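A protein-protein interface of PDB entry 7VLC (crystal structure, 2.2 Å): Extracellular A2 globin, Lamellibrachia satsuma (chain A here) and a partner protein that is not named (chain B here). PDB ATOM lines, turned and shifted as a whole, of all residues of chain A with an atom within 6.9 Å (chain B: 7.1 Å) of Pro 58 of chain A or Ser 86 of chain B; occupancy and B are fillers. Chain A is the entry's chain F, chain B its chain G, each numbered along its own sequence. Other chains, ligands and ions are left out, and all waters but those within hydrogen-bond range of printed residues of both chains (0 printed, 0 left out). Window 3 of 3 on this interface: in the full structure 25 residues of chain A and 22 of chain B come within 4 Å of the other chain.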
ATOM      1  N   VAL A  50     -26.669   5.484 -18.344  1.00  0.00           N
ATOM      2  CA  VAL A  50     -26.028   6.396 -17.403  1.00  0.00           C
ATOM      3  C   VAL A  50     -26.285   5.937 -15.972  1.00  0.00           C
ATOM      4  O   VAL A  50     -26.319   6.753 -15.045  1.00  0.00           O
ATOM      5  CB  VAL A  50     -26.517   7.840 -17.617  1.00  0.00           C
ATOM      6  CG1 VAL A  50     -26.098   8.335 -18.987  1.00  0.00           C
ATOM      7  CG2 VAL A  50     -28.027   7.919 -17.474  1.00  0.00           C
ATOM      8  N   ASN A  54     -28.441   3.550 -10.101  1.00  0.00           N
ATOM      9  CA  ASN A  54     -27.562   3.965  -9.006  1.00  0.00           C
ATOM     10  C   ASN A  54     -27.141   5.409  -9.289  1.00  0.00           C
ATOM     11  O   ASN A  54     -26.127   5.664  -9.945  1.00  0.00           O
ATOM     12  CB  ASN A  54     -26.361   3.030  -8.882  1.00  0.00           C
ATOM     13  CG  ASN A  54     -25.492   3.350  -7.683  1.00  0.00           C
ATOM     14  OD1 ASN A  54     -25.766   4.277  -6.923  1.00  0.00           O
ATOM     15  ND2 ASN A  54     -24.432   2.570  -7.507  1.00  0.00           N
ATOM     16  N   ILE A  55     -27.936   6.354  -8.771  1.00  0.00           N
ATOM     17  CA  ILE A  55     -27.670   7.774  -9.004  1.00  0.00           C
ATOM     18  C   ILE A  55     -26.495   8.306  -8.209  1.00  0.00           C
ATOM     19  O   ILE A  55     -26.150   9.488  -8.345  1.00  0.00           O
ATOM     20  CB  ILE A  55     -28.927   8.609  -8.703  1.00  0.00           C
ATOM     21  CG1 ILE A  55     -29.263   8.560  -7.207  1.00  0.00           C
ATOM     22  CG2 ILE A  55     -30.087   8.119  -9.522  1.00  0.00           C
ATOM     23  CD1 ILE A  55     -30.458   9.423  -6.848  1.00  0.00           C
ATOM     24  N   TYR A  56     -25.868   7.482  -7.366  1.00  0.00           N
ATOM     25  CA  TYR A  56     -24.644   7.843  -6.660  1.00  0.00           C
ATOM     26  C   TYR A  56     -23.379   7.640  -7.497  1.00  0.00           C
ATOM     27  O   TYR A  56     -22.288   8.060  -7.074  1.00  0.00           O
ATOM     28  CB  TYR A  56     -24.519   7.030  -5.367  1.00  0.00           C
ATOM     29  CG  TYR A  56     -25.728   7.121  -4.468  1.00  0.00           C
ATOM     30  CD1 TYR A  56     -26.785   6.221  -4.588  1.00  0.00           C
ATOM     31  CD2 TYR A  56     -25.810   8.097  -3.486  1.00  0.00           C
ATOM     32  CE1 TYR A  56     -27.888   6.299  -3.754  1.00  0.00           C
ATOM     33  CE2 TYR A  56     -26.905   8.185  -2.649  1.00  0.00           C
ATOM     34  CZ  TYR A  56     -27.943   7.284  -2.786  1.00  0.00           C
ATOM     35  OH  TYR A  56     -29.038   7.363  -1.952  1.00  0.00           O
ATOM     36  N   THR A  57     -23.498   7.002  -8.659  1.00  0.00           N
ATOM     37  CA  THR A  57     -22.346   6.734  -9.501  1.00  0.00           C
ATOM     38  C   THR A  57     -21.894   8.004 -10.215  1.00  0.00           C
ATOM     39  O   THR A  57     -22.708   8.888 -10.495  1.00  0.00           O
ATOM     40  CB  THR A  57     -22.682   5.667 -10.536  1.00  0.00           C
ATOM     41  OG1 THR A  57     -23.837   6.081 -11.277  1.00  0.00           O
ATOM     42  CG2 THR A  57     -22.943   4.326  -9.865  1.00  0.00           C
ATOM     43  N   PRO A  58     -20.598   8.113 -10.523  1.00  0.00           N
ATOM     44  CA  PRO A  58     -20.138   9.244 -11.338  1.00  0.00           C
ATOM     45  C   PRO A  58     -20.824   9.311 -12.685  1.00  0.00           C
ATOM     46  O   PRO A  58     -20.931  10.402 -13.259  1.00  0.00           O
ATOM     47  CB  PRO A  58     -18.632   8.986 -11.480  1.00  0.00           C
ATOM     48  CG  PRO A  58     -18.283   8.148 -10.308  1.00  0.00           C
ATOM     49  CD  PRO A  58     -19.479   7.270 -10.073  1.00  0.00           C
ATOM     50  N   ALA A  59     -21.302   8.175 -13.200  1.00  0.00           N
ATOM     51  CA  ALA A  59     -21.974   8.168 -14.495  1.00  0.00           C
ATOM     52  C   ALA A  59     -23.271   8.961 -14.442  1.00  0.00           C
ATOM     53  O   ALA A  59     -23.505   9.848 -15.272  1.00  0.00           O
ATOM     54  CB  ALA A  59     -22.242   6.730 -14.944  1.00  0.00           C
ATOM     55  N   PHE A  60     -24.129   8.663 -13.462  1.00  0.00           N
ATOM     56  CA  PHE A  60     -25.404   9.367 -13.392  1.00  0.00           C
ATOM     57  C   PHE A  60     -25.217  10.808 -12.934  1.00  0.00           C
ATOM     58  O   PHE A  60     -25.946  11.698 -13.381  1.00  0.00           O
ATOM     59  CB  PHE A  60     -26.387   8.646 -12.475  1.00  0.00           C
ATOM     60  CG  PHE A  60     -27.778   9.221 -12.537  1.00  0.00           C
ATOM     61  CD1 PHE A  60     -28.686   8.769 -13.480  1.00  0.00           C
ATOM     62  CD2 PHE A  60     -28.162  10.244 -11.684  1.00  0.00           C
ATOM     63  CE1 PHE A  60     -29.959   9.306 -13.555  1.00  0.00           C
ATOM     64  CE2 PHE A  60     -29.431  10.787 -11.754  1.00  0.00           C
ATOM     65  CZ  PHE A  60     -30.331  10.316 -12.690  1.00  0.00           C
ATOM     66  N   ARG A  61     -24.262  11.053 -12.033  1.00  0.00           N
ATOM     67  CA  ARG A  61     -24.014  12.422 -11.595  1.00  0.00           C
ATOM     68  C   ARG A  61     -23.601  13.298 -12.769  1.00  0.00           C
ATOM     69  O   ARG A  61     -23.959  14.480 -12.827  1.00  0.00           O
ATOM     70  CB  ARG A  61     -22.948  12.455 -10.498  1.00  0.00           C
ATOM     71  CG  ARG A  61     -23.351  11.776  -9.183  1.00  0.00           C
ATOM     72  CD  ARG A  61     -22.317  12.043  -8.097  1.00  0.00           C
ATOM     73  NE  ARG A  61     -22.472  11.163  -6.938  1.00  0.00           N
ATOM     74  CZ  ARG A  61     -23.291  11.404  -5.918  1.00  0.00           C
ATOM     75  NH1 ARG A  61     -23.362  10.551  -4.904  1.00  0.00           N
ATOM     76  NH2 ARG A  61     -24.043  12.494  -5.914  1.00  0.00           N
ATOM     77  N   ALA A  62     -22.871  12.726 -13.734  1.00  0.00           N
ATOM     78  CA  ALA A  62     -22.541  13.475 -14.940  1.00  0.00           C
ATOM     79  C   ALA A  62     -23.785  13.726 -15.775  1.00  0.00           C
ATOM     80  O   ALA A  62     -23.923  14.794 -16.381  1.00  0.00           O
ATOM     81  CB  ALA A  62     -21.480  12.736 -15.753  1.00  0.00           C
ATOM     82  N   HIS A  63     -24.706  12.761 -15.808  1.00  0.00           N
ATOM     83  CA  HIS A  63     -25.962  12.969 -16.519  1.00  0.00           C
ATOM     84  C   HIS A  63     -26.792  14.063 -15.859  1.00  0.00           C
ATOM     85  O   HIS A  63     -27.305  14.961 -16.538  1.00  0.00           O
ATOM     86  CB  HIS A  63     -26.758  11.667 -16.585  1.00  0.00           C
ATOM     87  CG  HIS A  63     -28.162  11.854 -17.068  1.00  0.00           C
ATOM     88  ND1 HIS A  63     -28.461  12.186 -18.371  1.00  0.00           N
ATOM     89  CD2 HIS A  63     -29.346  11.784 -16.416  1.00  0.00           C
ATOM     90  CE1 HIS A  63     -29.770  12.298 -18.504  1.00  0.00           C
ATOM     91  NE2 HIS A  63     -30.331  12.060 -17.332  1.00  0.00           N
ATOM     92  N   LEU B  81     -16.941  20.619 -12.310  1.00  0.00           N
ATOM     93  CA  LEU B  81     -16.625  19.244 -11.940  1.00  0.00           C
ATOM     94  C   LEU B  81     -15.144  19.016 -11.669  1.00  0.00           C
ATOM     95  O   LEU B  81     -14.763  17.891 -11.342  1.00  0.00           O
ATOM     96  CB  LEU B  81     -17.105  18.276 -13.023  1.00  0.00           C
ATOM     97  CG  LEU B  81     -18.618  18.066 -13.049  1.00  0.00           C
ATOM     98  CD1 LEU B  81     -19.007  17.107 -14.171  1.00  0.00           C
ATOM     99  CD2 LEU B  81     -19.120  17.574 -11.688  1.00  0.00           C
ATOM    100  N   SER B  83     -13.805  19.895  -9.094  1.00  0.00           N
ATOM    101  CA  SER B  83     -13.859  19.505  -7.689  1.00  0.00           C
ATOM    102  C   SER B  83     -14.200  18.033  -7.487  1.00  0.00           C
ATOM    103  O   SER B  83     -14.031  17.526  -6.374  1.00  0.00           O
ATOM    104  CB  SER B  83     -14.891  20.359  -6.947  1.00  0.00           C
ATOM    105  OG  SER B  83     -14.701  21.734  -7.214  1.00  0.00           O
ATOM    106  N   ASP B  84     -14.696  17.345  -8.513  1.00  0.00           N
ATOM    107  CA  ASP B  84     -15.065  15.932  -8.417  1.00  0.00           C
ATOM    108  C   ASP B  84     -14.593  15.241  -9.683  1.00  0.00           C
ATOM    109  O   ASP B  84     -15.374  15.005 -10.612  1.00  0.00           O
ATOM    110  CB  ASP B  84     -16.572  15.761  -8.220  1.00  0.00           C
ATOM    111  CG  ASP B  84     -16.977  14.303  -8.030  1.00  0.00           C
ATOM    112  OD1 ASP B  84     -16.112  13.481  -7.658  1.00  0.00           O
ATOM    113  OD2 ASP B  84     -18.159  13.978  -8.263  1.00  0.00           O
ATOM    114  N   PRO B  85     -13.306  14.906  -9.758  1.00  0.00           N
ATOM    115  CA  PRO B  85     -12.763  14.378 -11.022  1.00  0.00           C
ATOM    116  C   PRO B  85     -13.390  13.066 -11.463  1.00  0.00           C
ATOM    117  O   PRO B  85     -13.425  12.795 -12.670  1.00  0.00           O
ATOM    118  CB  PRO B  85     -11.264  14.224 -10.716  1.00  0.00           C
ATOM    119  CG  PRO B  85     -11.003  15.181  -9.599  1.00  0.00           C
ATOM    120  CD  PRO B  85     -12.250  15.147  -8.758  1.00  0.00           C
ATOM    121  N   SER B  86     -13.886  12.245 -10.532  1.00  0.00           N
ATOM    122  CA  SER B  86     -14.586  11.020 -10.915  1.00  0.00           C
ATOM    123  C   SER B  86     -15.751  11.330 -11.843  1.00  0.00           C
ATOM    124  O   SER B  86     -15.878  10.740 -12.923  1.00  0.00           O
ATOM    125  CB  SER B  86     -15.081  10.276  -9.674  1.00  0.00           C
ATOM    126  OG  SER B  86     -14.002   9.923  -8.831  1.00  0.00           O
ATOM    127  N   THR B  87     -16.611  12.266 -11.436  1.00  0.00           N
ATOM    128  CA  THR B  87     -17.718  12.678 -12.290  1.00  0.00           C
ATOM    129  C   THR B  87     -17.227  13.454 -13.504  1.00  0.00           C
ATOM    130  O   THR B  87     -17.814  13.345 -14.587  1.00  0.00           O
ATOM    131  CB  THR B  87     -18.713  13.510 -11.482  1.00  0.00           C
ATOM    132  OG1 THR B  87     -19.101  12.772 -10.314  1.00  0.00           O
ATOM    133  CG2 THR B  87     -19.952  13.822 -12.309  1.00  0.00           C
ATOM    134  N   LEU B  88     -16.143  14.223 -13.350  1.00  0.00           N
ATOM    135  CA  LEU B  88     -15.589  14.967 -14.475  1.00  0.00           C
ATOM    136  C   LEU B  88     -15.195  14.036 -15.617  1.00  0.00           C
ATOM    137  O   LEU B  88     -15.495  14.313 -16.783  1.00  0.00           O
ATOM    138  CB  LEU B  88     -14.385  15.786 -14.017  1.00  0.00           C
ATOM    139  CG  LEU B  88     -13.568  16.466 -15.121  1.00  0.00           C
ATOM    140  CD1 LEU B  88     -14.351  17.604 -15.767  1.00  0.00           C
ATOM    141  CD2 LEU B  88     -12.231  16.961 -14.588  1.00  0.00           C
ATOM    142  N   ASN B  89     -14.527  12.923 -15.298  1.00  0.00           N
ATOM    143  CA  ASN B  89     -14.113  11.983 -16.338  1.00  0.00           C
ATOM    144  C   ASN B  89     -15.311  11.481 -17.132  1.00  0.00           C
ATOM    145  O   ASN B  89     -15.222  11.294 -18.350  1.00  0.00           O
ATOM    146  CB  ASN B  89     -13.345  10.814 -15.721  1.00  0.00           C
ATOM    147  CG  ASN B  89     -11.994  11.224 -15.170  1.00  0.00           C
ATOM    148  OD1 ASN B  89     -11.336  12.119 -15.705  1.00  0.00           O
ATOM    149  ND2 ASN B  89     -11.569  10.566 -14.096  1.00  0.00           N
ATOM    150  N   GLU B  90     -16.447  11.275 -16.462  1.00  0.00           N
ATOM    151  CA  GLU B  90     -17.654  10.834 -17.155  1.00  0.00           C
ATOM    152  C   GLU B  90     -18.213  11.930 -18.053  1.00  0.00           C
ATOM    153  O   GLU B  90     -18.685  11.651 -19.161  1.00  0.00           O
ATOM    154  CB  GLU B  90     -18.706  10.381 -16.144  1.00  0.00           C
ATOM    155  CG  GLU B  90     -18.346   9.084 -15.456  1.00  0.00           C
ATOM    156  CD  GLU B  90     -18.078   7.969 -16.454  1.00  0.00           C
ATOM    157  OE1 GLU B  90     -18.934   7.736 -17.335  1.00  0.00           O
ATOM    158  OE2 GLU B  90     -17.003   7.344 -16.368  1.00  0.00           O
ATOM    159  N   GLN B  91     -18.181  13.181 -17.588  1.00  0.00           N
ATOM    160  CA  GLN B  91     -18.673  14.286 -18.404  1.00  0.00           C
ATOM    161  C   GLN B  91     -17.765  14.535 -19.600  1.00  0.00           C
ATOM    162  O   GLN B  91     -18.247  14.808 -20.706  1.00  0.00           O
ATOM    163  CB  GLN B  91     -18.796  15.551 -17.556  1.00  0.00           C
ATOM    164  CG  GLN B  91     -19.170  16.797 -18.341  1.00  0.00           C
ATOM    165  CD  GLN B  91     -20.619  16.805 -18.782  1.00  0.00           C
ATOM    166  OE1 GLN B  91     -21.389  15.898 -18.456  1.00  0.00           O
ATOM    167  NE2 GLN B  91     -21.003  17.837 -19.525  1.00  0.00           N
ATOM    168  N   ARG B 139      -6.171  20.144 -19.047  1.00  0.00           N
ATOM    169  CA  ARG B 139      -6.692  18.955 -18.381  1.00  0.00           C
ATOM    170  C   ARG B 139      -8.105  18.642 -18.846  1.00  0.00           C
ATOM    171  O   ARG B 139      -8.488  17.471 -18.927  1.00  0.00           O
ATOM    172  CB  ARG B 139      -6.645  19.153 -16.862  1.00  0.00           C
ATOM    173  CG  ARG B 139      -7.534  18.212 -16.046  1.00  0.00           C
ATOM    174  CD  ARG B 139      -7.033  16.779 -16.079  1.00  0.00           C
ATOM    175  NE  ARG B 139      -7.863  15.890 -15.269  1.00  0.00           N
ATOM    176  CZ  ARG B 139      -8.878  15.175 -15.745  1.00  0.00           C
ATOM    177  NH1 ARG B 139      -9.192  15.239 -17.030  1.00  0.00           N
ATOM    178  NH2 ARG B 139      -9.579  14.391 -14.934  1.00  0.00           N
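The backbone carbonyl oxygen (O) of Ala 62 of chain A lies close to the side-chain amide oxygen (OE1) of Gln 91 of chain B (3.5 Å).
The backbone carbonyl oxygen of Tyr 56 of chain A sits at hydrogen-bond distance from the guanidinium group of Arg 61 of chain A (3.1 Å). OD2 of Asp 84 of chain B is in hydrogen-bond range of OG1 of Thr 87 of chain B (2.6 Å).
Among the printed residues, merely in contact across the chains: Ala 62 of chain A with Thr 87 of chain B, Pro 58 of chain A with Ser 86 of chain B, Pro 58 of chain A with Glu 90 of chain B, Ala 62 of chain A with Glu 90 of chain B, Pro 58 of chain A with Thr 87 of chain B, Arg 61 of chain A with Thr 87 of chain B and Ala 59 of chain A with Glu 90 of chain B.
Pro 58 of chain A touches just these residues of chain B: Ser 86 (3.6 Å), Thr 87 (3.7 Å) and Glu 90 (3.6 Å). Printed residues of chain B within 4 Å of Ala 59 of chain A: Glu 90. Of the printed residues of chain B, Arg 61 of chain A touches Thr 87 (3.7 Å). Of the printed residues of chain B, Ala 62 of chain A touches Thr 87, Glu 90 and Gln 91. Ser 86 of chain B touches just one residue of chain A: Pro 58 (3.6 Å). Leu 88 of chain B touches none of the printed residues of chain A. Printed residues of chain A within 4 Å of Glu 90 of chain B: Pro 58, Ala 59 and Ala 62. Of the printed residues of chain A, Gln 91 of chain B touches Ala 62. The nearest printed residue of chain B that does not touch Ala 59 of chain A is Thr 87 of chain B (5.8 Å).
Of the 11 printed residues of chain B, 4 touch a printed residue of chain A. Printed residues of chain A that touch a printed residue of chain B: Pro 58, Ala 59, Arg 61 and Ala 62. Among the printed residues, no Asp or Glu carboxylate lies within 4 Å of a Lys or Arg side-chain nitrogen of the other chain.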
